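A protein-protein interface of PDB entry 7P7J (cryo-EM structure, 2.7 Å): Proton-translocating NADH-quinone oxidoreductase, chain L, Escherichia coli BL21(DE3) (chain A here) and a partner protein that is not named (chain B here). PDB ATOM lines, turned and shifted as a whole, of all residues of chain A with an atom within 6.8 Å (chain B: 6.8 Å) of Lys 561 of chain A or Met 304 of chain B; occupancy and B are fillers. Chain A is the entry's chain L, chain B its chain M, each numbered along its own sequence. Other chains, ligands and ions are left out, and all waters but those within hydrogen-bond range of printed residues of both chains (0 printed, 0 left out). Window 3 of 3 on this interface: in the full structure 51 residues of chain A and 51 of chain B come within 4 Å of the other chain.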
ATOM      1  N   ILE A 556     -18.750  12.639   6.614  1.00  0.00           N
ATOM      2  CA  ILE A 556     -17.439  12.230   6.128  1.00  0.00           C
ATOM      3  C   ILE A 556     -16.605  11.654   7.265  1.00  0.00           C
ATOM      4  O   ILE A 556     -15.879  10.671   7.078  1.00  0.00           O
ATOM      5  CB  ILE A 556     -16.743  13.416   5.431  1.00  0.00           C
ATOM      6  CG1 ILE A 556     -17.397  13.688   4.078  1.00  0.00           C
ATOM      7  CG2 ILE A 556     -15.267  13.150   5.207  1.00  0.00           C
ATOM      8  CD1 ILE A 556     -16.896  14.941   3.406  1.00  0.00           C
ATOM      9  N   ALA A 557     -16.720  12.227   8.468  1.00  0.00           N
ATOM     10  CA  ALA A 557     -16.012  11.671   9.618  1.00  0.00           C
ATOM     11  C   ALA A 557     -16.503  10.267   9.952  1.00  0.00           C
ATOM     12  O   ALA A 557     -15.697   9.366  10.220  1.00  0.00           O
ATOM     13  CB  ALA A 557     -16.167  12.594  10.826  1.00  0.00           C
ATOM     14  N   TRP A 558     -17.822  10.056   9.920  1.00  0.00           N
ATOM     15  CA  TRP A 558     -18.367   8.727  10.185  1.00  0.00           C
ATOM     16  C   TRP A 558     -17.979   7.739   9.093  1.00  0.00           C
ATOM     17  O   TRP A 558     -17.730   6.561   9.374  1.00  0.00           O
ATOM     18  CB  TRP A 558     -19.888   8.802  10.326  1.00  0.00           C
ATOM     19  CG  TRP A 558     -20.535   7.464  10.489  1.00  0.00           C
ATOM     20  CD1 TRP A 558     -20.708   6.773  11.651  1.00  0.00           C
ATOM     21  CD2 TRP A 558     -21.093   6.650   9.451  1.00  0.00           C
ATOM     22  NE1 TRP A 558     -21.340   5.580  11.402  1.00  0.00           N
ATOM     23  CE2 TRP A 558     -21.586   5.480  10.058  1.00  0.00           C
ATOM     24  CE3 TRP A 558     -21.221   6.798   8.067  1.00  0.00           C
ATOM     25  CZ2 TRP A 558     -22.200   4.466   9.330  1.00  0.00           C
ATOM     26  CZ3 TRP A 558     -21.830   5.790   7.346  1.00  0.00           C
ATOM     27  CH2 TRP A 558     -22.312   4.638   7.978  1.00  0.00           C
ATOM     28  N   LEU A 559     -17.928   8.198   7.843  1.00  0.00           N
ATOM     29  CA  LEU A 559     -17.521   7.331   6.744  1.00  0.00           C
ATOM     30  C   LEU A 559     -16.043   6.972   6.824  1.00  0.00           C
ATOM     31  O   LEU A 559     -15.659   5.851   6.472  1.00  0.00           O
ATOM     32  CB  LEU A 559     -17.842   8.013   5.414  1.00  0.00           C
ATOM     33  CG  LEU A 559     -17.526   7.280   4.112  1.00  0.00           C
ATOM     34  CD1 LEU A 559     -18.741   7.287   3.204  1.00  0.00           C
ATOM     35  CD2 LEU A 559     -16.342   7.929   3.420  1.00  0.00           C
ATOM     36  N   LEU A 560     -15.204   7.896   7.286  1.00  0.00           N
ATOM     37  CA  LEU A 560     -13.766   7.687   7.321  1.00  0.00           C
ATOM     38  C   LEU A 560     -13.264   7.095   8.629  1.00  0.00           C
ATOM     39  O   LEU A 560     -12.082   6.752   8.703  1.00  0.00           O
ATOM     40  CB  LEU A 560     -13.030   9.005   7.065  1.00  0.00           C
ATOM     41  CG  LEU A 560     -13.059   9.558   5.641  1.00  0.00           C
ATOM     42  CD1 LEU A 560     -12.093  10.722   5.507  1.00  0.00           C
ATOM     43  CD2 LEU A 560     -12.739   8.473   4.631  1.00  0.00           C
ATOM     44  N   LYS A 561     -14.120   6.950   9.646  1.00  0.00           N
ATOM     45  CA  LYS A 561     -13.668   6.474  10.954  1.00  0.00           C
ATOM     46  C   LYS A 561     -13.082   5.064  10.926  1.00  0.00           C
ATOM     47  O   LYS A 561     -12.384   4.683  11.872  1.00  0.00           O
ATOM     48  CB  LYS A 561     -14.820   6.526  11.959  1.00  0.00           C
ATOM     49  CG  LYS A 561     -15.837   5.414  11.807  1.00  0.00           C
ATOM     50  CD  LYS A 561     -16.926   5.520  12.856  1.00  0.00           C
ATOM     51  CE  LYS A 561     -17.949   4.410  12.696  1.00  0.00           C
ATOM     52  NZ  LYS A 561     -19.066   4.546  13.668  1.00  0.00           N
ATOM     53  N   ARG A 562     -13.336   4.285   9.877  1.00  0.00           N
ATOM     54  CA  ARG A 562     -12.726   2.969   9.739  1.00  0.00           C
ATOM     55  C   ARG A 562     -11.342   3.017   9.101  1.00  0.00           C
ATOM     56  O   ARG A 562     -10.722   1.958   8.952  1.00  0.00           O
ATOM     57  CB  ARG A 562     -13.633   2.050   8.919  1.00  0.00           C
ATOM     58  CG  ARG A 562     -13.803   2.478   7.470  1.00  0.00           C
ATOM     59  CD  ARG A 562     -14.594   1.447   6.677  1.00  0.00           C
ATOM     60  NE  ARG A 562     -13.752   0.705   5.746  1.00  0.00           N
ATOM     61  CZ  ARG A 562     -13.437  -0.576   5.874  1.00  0.00           C
ATOM     62  NH1 ARG A 562     -13.873  -1.296   6.895  1.00  0.00           N
ATOM     63  NH2 ARG A 562     -12.664  -1.150   4.957  1.00  0.00           N
ATOM     64  N   ASP A 563     -10.857   4.211   8.718  1.00  0.00           N
ATOM     65  CA  ASP A 563      -9.560   4.456   8.085  1.00  0.00           C
ATOM     66  C   ASP A 563      -9.417   3.653   6.794  1.00  0.00           C
ATOM     67  O   ASP A 563      -8.686   2.655   6.771  1.00  0.00           O
ATOM     68  CB  ASP A 563      -8.416   4.135   9.052  1.00  0.00           C
ATOM     69  CG  ASP A 563      -7.151   4.912   8.743  1.00  0.00           C
ATOM     70  OD1 ASP A 563      -7.099   5.579   7.692  1.00  0.00           O
ATOM     71  OD2 ASP A 563      -6.205   4.855   9.555  1.00  0.00           O
ATOM     72  N   PRO A 564     -10.119   4.036   5.720  1.00  0.00           N
ATOM     73  CA  PRO A 564     -10.097   3.223   4.488  1.00  0.00           C
ATOM     74  C   PRO A 564      -8.732   3.097   3.831  1.00  0.00           C
ATOM     75  O   PRO A 564      -8.457   2.065   3.204  1.00  0.00           O
ATOM     76  CB  PRO A 564     -11.088   3.957   3.571  1.00  0.00           C
ATOM     77  CG  PRO A 564     -11.906   4.809   4.478  1.00  0.00           C
ATOM     78  CD  PRO A 564     -10.991   5.212   5.579  1.00  0.00           C
ATOM     79  N   HIS B 241       0.383   5.523   6.408  1.00  0.00           N
ATOM     80  CA  HIS B 241       0.350   6.244   7.674  1.00  0.00           C
ATOM     81  C   HIS B 241      -0.130   5.407   8.853  1.00  0.00           C
ATOM     82  O   HIS B 241       0.252   5.689   9.991  1.00  0.00           O
ATOM     83  CB  HIS B 241      -0.539   7.479   7.538  1.00  0.00           C
ATOM     84  CG  HIS B 241      -1.978   7.152   7.305  1.00  0.00           C
ATOM     85  ND1 HIS B 241      -2.476   6.839   6.060  1.00  0.00           N
ATOM     86  CD2 HIS B 241      -3.026   7.073   8.159  1.00  0.00           C
ATOM     87  CE1 HIS B 241      -3.769   6.588   6.155  1.00  0.00           C
ATOM     88  NE2 HIS B 241      -4.127   6.723   7.419  1.00  0.00           N
ATOM     89  N   PHE B 299      -6.100  17.065   5.480  1.00  0.00           N
ATOM     90  CA  PHE B 299      -7.545  16.894   5.613  1.00  0.00           C
ATOM     91  C   PHE B 299      -7.899  15.518   6.166  1.00  0.00           C
ATOM     92  O   PHE B 299      -8.767  15.396   7.040  1.00  0.00           O
ATOM     93  CB  PHE B 299      -8.225  17.124   4.268  1.00  0.00           C
ATOM     94  CG  PHE B 299      -8.687  18.532   4.061  1.00  0.00           C
ATOM     95  CD1 PHE B 299      -7.934  19.593   4.530  1.00  0.00           C
ATOM     96  CD2 PHE B 299      -9.875  18.798   3.403  1.00  0.00           C
ATOM     97  CE1 PHE B 299      -8.351  20.891   4.345  1.00  0.00           C
ATOM     98  CE2 PHE B 299     -10.301  20.098   3.214  1.00  0.00           C
ATOM     99  CZ  PHE B 299      -9.535  21.147   3.688  1.00  0.00           C
ATOM    100  N   TYR B 300      -7.225  14.476   5.677  1.00  0.00           N
ATOM    101  CA  TYR B 300      -7.481  13.117   6.127  1.00  0.00           C
ATOM    102  C   TYR B 300      -7.089  12.930   7.584  1.00  0.00           C
ATOM    103  O   TYR B 300      -7.810  12.271   8.336  1.00  0.00           O
ATOM    104  CB  TYR B 300      -6.726  12.136   5.234  1.00  0.00           C
ATOM    105  CG  TYR B 300      -7.106  10.695   5.438  1.00  0.00           C
ATOM    106  CD1 TYR B 300      -8.259  10.174   4.868  1.00  0.00           C
ATOM    107  CD2 TYR B 300      -6.312   9.852   6.197  1.00  0.00           C
ATOM    108  CE1 TYR B 300      -8.608   8.856   5.052  1.00  0.00           C
ATOM    109  CE2 TYR B 300      -6.652   8.536   6.388  1.00  0.00           C
ATOM    110  CZ  TYR B 300      -7.800   8.043   5.813  1.00  0.00           C
ATOM    111  OH  TYR B 300      -8.139   6.727   6.003  1.00  0.00           O
ATOM    112  N   GLY B 301      -5.958  13.502   8.004  1.00  0.00           N
ATOM    113  CA  GLY B 301      -5.566  13.405   9.397  1.00  0.00           C
ATOM    114  C   GLY B 301      -6.504  14.157  10.316  1.00  0.00           C
ATOM    115  O   GLY B 301      -6.783  13.705  11.427  1.00  0.00           O
ATOM    116  N   ALA B 302      -7.017  15.306   9.865  1.00  0.00           N
ATOM    117  CA  ALA B 302      -7.982  16.038  10.678  1.00  0.00           C
ATOM    118  C   ALA B 302      -9.294  15.274  10.826  1.00  0.00           C
ATOM    119  O   ALA B 302      -9.838  15.173  11.934  1.00  0.00           O
ATOM    120  CB  ALA B 302      -8.225  17.416  10.074  1.00  0.00           C
ATOM    121  N   TRP B 303      -9.811  14.722   9.724  1.00  0.00           N
ATOM    122  CA  TRP B 303     -11.037  13.931   9.797  1.00  0.00           C
ATOM    123  C   TRP B 303     -10.833  12.654  10.600  1.00  0.00           C
ATOM    124  O   TRP B 303     -11.749  12.197  11.293  1.00  0.00           O
ATOM    125  CB  TRP B 303     -11.534  13.602   8.394  1.00  0.00           C
ATOM    126  CG  TRP B 303     -12.573  14.539   7.894  1.00  0.00           C
ATOM    127  CD1 TRP B 303     -13.696  14.935   8.551  1.00  0.00           C
ATOM    128  CD2 TRP B 303     -12.590  15.201   6.628  1.00  0.00           C
ATOM    129  NE1 TRP B 303     -14.417  15.803   7.770  1.00  0.00           N
ATOM    130  CE2 TRP B 303     -13.756  15.985   6.584  1.00  0.00           C
ATOM    131  CE3 TRP B 303     -11.732  15.206   5.525  1.00  0.00           C
ATOM    132  CZ2 TRP B 303     -14.089  16.765   5.482  1.00  0.00           C
ATOM    133  CZ3 TRP B 303     -12.063  15.983   4.434  1.00  0.00           C
ATOM    134  CH2 TRP B 303     -13.229  16.753   4.421  1.00  0.00           C
ATOM    135  N   MET B 304      -9.645  12.059  10.505  1.00  0.00           N
ATOM    136  CA  MET B 304      -9.316  10.890  11.307  1.00  0.00           C
ATOM    137  C   MET B 304      -9.269  11.233  12.787  1.00  0.00           C
ATOM    138  O   MET B 304      -9.777  10.476  13.620  1.00  0.00           O
ATOM    139  CB  MET B 304      -7.969  10.330  10.854  1.00  0.00           C
ATOM    140  CG  MET B 304      -7.963   9.264   9.755  1.00  0.00           C
ATOM    141  SD  MET B 304      -9.420   8.266   9.395  1.00  0.00           S
ATOM    142  CE  MET B 304      -9.727   7.386  10.932  1.00  0.00           C
ATOM    143  N   ALA B 305      -8.660  12.371  13.128  1.00  0.00           N
ATOM    144  CA  ALA B 305      -8.530  12.774  14.521  1.00  0.00           C
ATOM    145  C   ALA B 305      -9.883  13.107  15.131  1.00  0.00           C
ATOM    146  O   ALA B 305     -10.131  12.794  16.299  1.00  0.00           O
ATOM    147  CB  ALA B 305      -7.582  13.966  14.631  1.00  0.00           C
ATOM    148  N   PHE B 306     -10.768  13.745  14.362  1.00  0.00           N
ATOM    149  CA  PHE B 306     -12.098  14.032  14.887  1.00  0.00           C
ATOM    150  C   PHE B 306     -12.905  12.761  15.117  1.00  0.00           C
ATOM    151  O   PHE B 306     -13.720  12.706  16.043  1.00  0.00           O
ATOM    152  CB  PHE B 306     -12.858  14.965  13.949  1.00  0.00           C
ATOM    153  CG  PHE B 306     -14.240  15.298  14.428  1.00  0.00           C
ATOM    154  CD1 PHE B 306     -14.426  16.174  15.480  1.00  0.00           C
ATOM    155  CD2 PHE B 306     -15.353  14.723  13.838  1.00  0.00           C
ATOM    156  CE1 PHE B 306     -15.691  16.477  15.931  1.00  0.00           C
ATOM    157  CE2 PHE B 306     -16.620  15.023  14.286  1.00  0.00           C
ATOM    158  CZ  PHE B 306     -16.789  15.901  15.333  1.00  0.00           C
ATOM    159  N   ALA B 307     -12.687  11.731  14.300  1.00  0.00           N
ATOM    160  CA  ALA B 307     -13.467  10.502  14.366  1.00  0.00           C
ATOM    161  C   ALA B 307     -12.839   9.449  15.270  1.00  0.00           C
ATOM    162  O   ALA B 307     -13.106   8.253  15.094  1.00  0.00           O
ATOM    163  CB  ALA B 307     -13.673   9.939  12.961  1.00  0.00           C
ATOM    164  N   GLN B 308     -12.022   9.852  16.234  1.00  0.00           N
ATOM    165  CA  GLN B 308     -11.358   8.914  17.126  1.00  0.00           C
ATOM    166  C   GLN B 308     -12.044   8.888  18.483  1.00  0.00           C
ATOM    167  O   GLN B 308     -12.391   9.934  19.036  1.00  0.00           O
ATOM    168  CB  GLN B 308      -9.883   9.271  17.316  1.00  0.00           C
ATOM    169  CG  GLN B 308      -8.955   8.769  16.222  1.00  0.00           C
ATOM    170  CD  GLN B 308      -9.363   7.425  15.658  1.00  0.00           C
ATOM    171  OE1 GLN B 308      -9.449   6.432  16.377  1.00  0.00           O
ATOM    172  NE2 GLN B 308      -9.622   7.388  14.358  1.00  0.00           N
ATOM    173  N   THR B 309     -12.250   7.683  19.004  1.00  0.00           N
ATOM    174  CA  THR B 309     -12.667   7.500  20.386  1.00  0.00           C
ATOM    175  C   THR B 309     -11.486   7.299  21.324  1.00  0.00           C
ATOM    176  O   THR B 309     -11.682   7.230  22.541  1.00  0.00           O
ATOM    177  CB  THR B 309     -13.618   6.306  20.500  1.00  0.00           C
ATOM    178  OG1 THR B 309     -12.898   5.097  20.239  1.00  0.00           O
ATOM    179  CG2 THR B 309     -14.749   6.436  19.496  1.00  0.00           C
ATOM    180  N   ARG B 313      -4.736   7.826  19.688  1.00  0.00           N
ATOM    181  CA  ARG B 313      -4.937   7.807  18.244  1.00  0.00           C
ATOM    182  C   ARG B 313      -5.238   9.201  17.706  1.00  0.00           C
ATOM    183  O   ARG B 313      -4.810   9.548  16.596  1.00  0.00           O
ATOM    184  CB  ARG B 313      -6.064   6.836  17.903  1.00  0.00           C
ATOM    185  CG  ARG B 313      -5.908   6.130  16.574  1.00  0.00           C
ATOM    186  CD  ARG B 313      -6.683   4.825  16.547  1.00  0.00           C
ATOM    187  NE  ARG B 313      -5.873   3.687  16.955  1.00  0.00           N
ATOM    188  CZ  ARG B 313      -5.324   2.828  16.109  1.00  0.00           C
ATOM    189  NH1 ARG B 313      -5.482   2.953  14.801  1.00  0.00           N
ATOM    190  NH2 ARG B 313      -4.602   1.819  16.584  1.00  0.00           N
ATOM    191  N   LEU B 314      -5.956  10.013  18.486  1.00  0.00           N
ATOM    192  CA  LEU B 314      -6.226  11.394  18.099  1.00  0.00           C
ATOM    193  C   LEU B 314      -4.940  12.204  17.991  1.00  0.00           C
ATOM    194  O   LEU B 314      -4.757  12.968  17.034  1.00  0.00           O
ATOM    195  CB  LEU B 314      -7.181  12.030  19.109  1.00  0.00           C
ATOM    196  CG  LEU B 314      -7.898  13.335  18.774  1.00  0.00           C
ATOM    197  CD1 LEU B 314      -9.279  13.303  19.378  1.00  0.00           C
ATOM    198  CD2 LEU B 314      -7.131  14.541  19.288  1.00  0.00           C
ATOM    199  N   TYR B 317      -3.081  11.163  14.818  1.00  0.00           N
ATOM    200  CA  TYR B 317      -3.599  11.751  13.585  1.00  0.00           C
ATOM    201  C   TYR B 317      -3.354  13.258  13.526  1.00  0.00           C
ATOM    202  O   TYR B 317      -3.220  13.826  12.430  1.00  0.00           O
ATOM    203  CB  TYR B 317      -5.077  11.417  13.442  1.00  0.00           C
ATOM    204  CG  TYR B 317      -5.314   9.980  13.038  1.00  0.00           C
ATOM    205  CD1 TYR B 317      -4.696   9.447  11.915  1.00  0.00           C
ATOM    206  CD2 TYR B 317      -6.150   9.158  13.776  1.00  0.00           C
ATOM    207  CE1 TYR B 317      -4.912   8.138  11.538  1.00  0.00           C
ATOM    208  CE2 TYR B 317      -6.366   7.848  13.408  1.00  0.00           C
ATOM    209  CZ  TYR B 317      -5.746   7.343  12.290  1.00  0.00           C
ATOM    210  OH  TYR B 317      -5.963   6.038  11.924  1.00  0.00           O
ATOM    211  N   TYR B 435     -10.849  19.669  15.659  1.00  0.00           N
ATOM    212  CA  TYR B 435     -10.583  18.422  16.381  1.00  0.00           C
ATOM    213  C   TYR B 435      -9.934  18.672  17.740  1.00  0.00           C
ATOM    214  O   TYR B 435     -10.155  17.890  18.674  1.00  0.00           O
ATOM    215  CB  TYR B 435      -9.767  17.421  15.539  1.00  0.00           C
ATOM    216  CG  TYR B 435      -8.334  17.739  15.124  1.00  0.00           C
ATOM    217  CD1 TYR B 435      -7.307  17.884  16.054  1.00  0.00           C
ATOM    218  CD2 TYR B 435      -8.000  17.803  13.785  1.00  0.00           C
ATOM    219  CE1 TYR B 435      -6.016  18.151  15.658  1.00  0.00           C
ATOM    220  CE2 TYR B 435      -6.709  18.044  13.380  1.00  0.00           C
ATOM    221  CZ  TYR B 435      -5.725  18.231  14.317  1.00  0.00           C
ATOM    222  OH  TYR B 435      -4.443  18.487  13.899  1.00  0.00           O
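The backbone nitrogen (N) of Pro 564 of chain A lies close to the side-chain hydroxyl (OH) of Tyr 300 of chain B (3.4 Å). The side-chain carboxylate (OD1) of Asp 563 of chain A is in hydrogen-bond range of a ring nitrogen (NE2) of His 241 of chain B. The side-chain hydroxyl (OH) of Tyr 317 of chain B is in hydrogen-bond range of the side-chain carboxylate (OD2) of Asp 563 of chain A, 2.7 Å away. SD of Met 304 of chain B lies close to O of Leu 560 of chain A (3.1 Å). The side-chain hydroxyl of Tyr 300 of chain B sits close to the side-chain carboxylate of Asp 563 of chain A (2.3 Å).
The backbone carbonyl oxygen of Met 304 of chain B is in hydrogen-bond range of the side-chain amide nitrogen of Gln 308 of chain B (3.2 Å).
Among the printed residues, merely in contact across the chains: Ile 556 of chain A with Trp 303 of chain B (3.5 Å), Ala 557 of chain A with Phe 306 of chain B (3.8 Å), Ala 557 of chain A with Ala 307 of chain B (3.5 Å), Leu 560 of chain A with Tyr 300 of chain B (3.9 Å), Lys 561 of chain A with Met 304 of chain B (3.9 Å), Lys 561 of chain A with Ala 307 of chain B (3.7 Å) and Asp 563 of chain A with Met 304 of chain B (3.9 Å).
Of the printed residues of chain B, Ala 557 of chain A touches Phe 306 and Ala 307. Trp 558 of chain A touches none of the printed residues of chain B. Leu 559 of chain A touches none of the printed residues of chain B. Lys 561 of chain A touches just these residues of chain B: Met 304 (3.9 Å) and Ala 307 (3.7 Å). Printed residues of chain A within 4 Å of Met 304 of chain B: Leu 560 (3.1 Å), Lys 561 (3.9 Å) and Asp 563 (3.9 Å). Of the printed residues of chain A, Ala 307 of chain B touches Ala 557 (3.5 Å) and Lys 561 (3.7 Å). The nearest residue of chain B that does not touch Lys 561 of chain A is Gln 308 of chain B (4.6 Å).
Of the 9 printed residues of chain A, 6 touch a printed residue of chain B. Hydrophobic or aromatic side chains of chain A within 4 Å of the printed part of chain B: Ile 556, Ala 557, Leu 560 and Pro 564. Of the 16 printed residues of chain B, 7 touch a printed residue of chain A. Hydrophobic or aromatic side chains of chain B within 4 Å of the printed part of chain A: His 241, Tyr 300, Trp 303, Met 304, Phe 306, Ala 307 and Tyr 317. Along chain B the printed residues that touch a printed residue of chain A span positions 241 to 317. Among the printed residues, no Asp or Glu carboxylate lies within 4 Å of a Lys or Arg side-chain nitrogen of the other chain.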
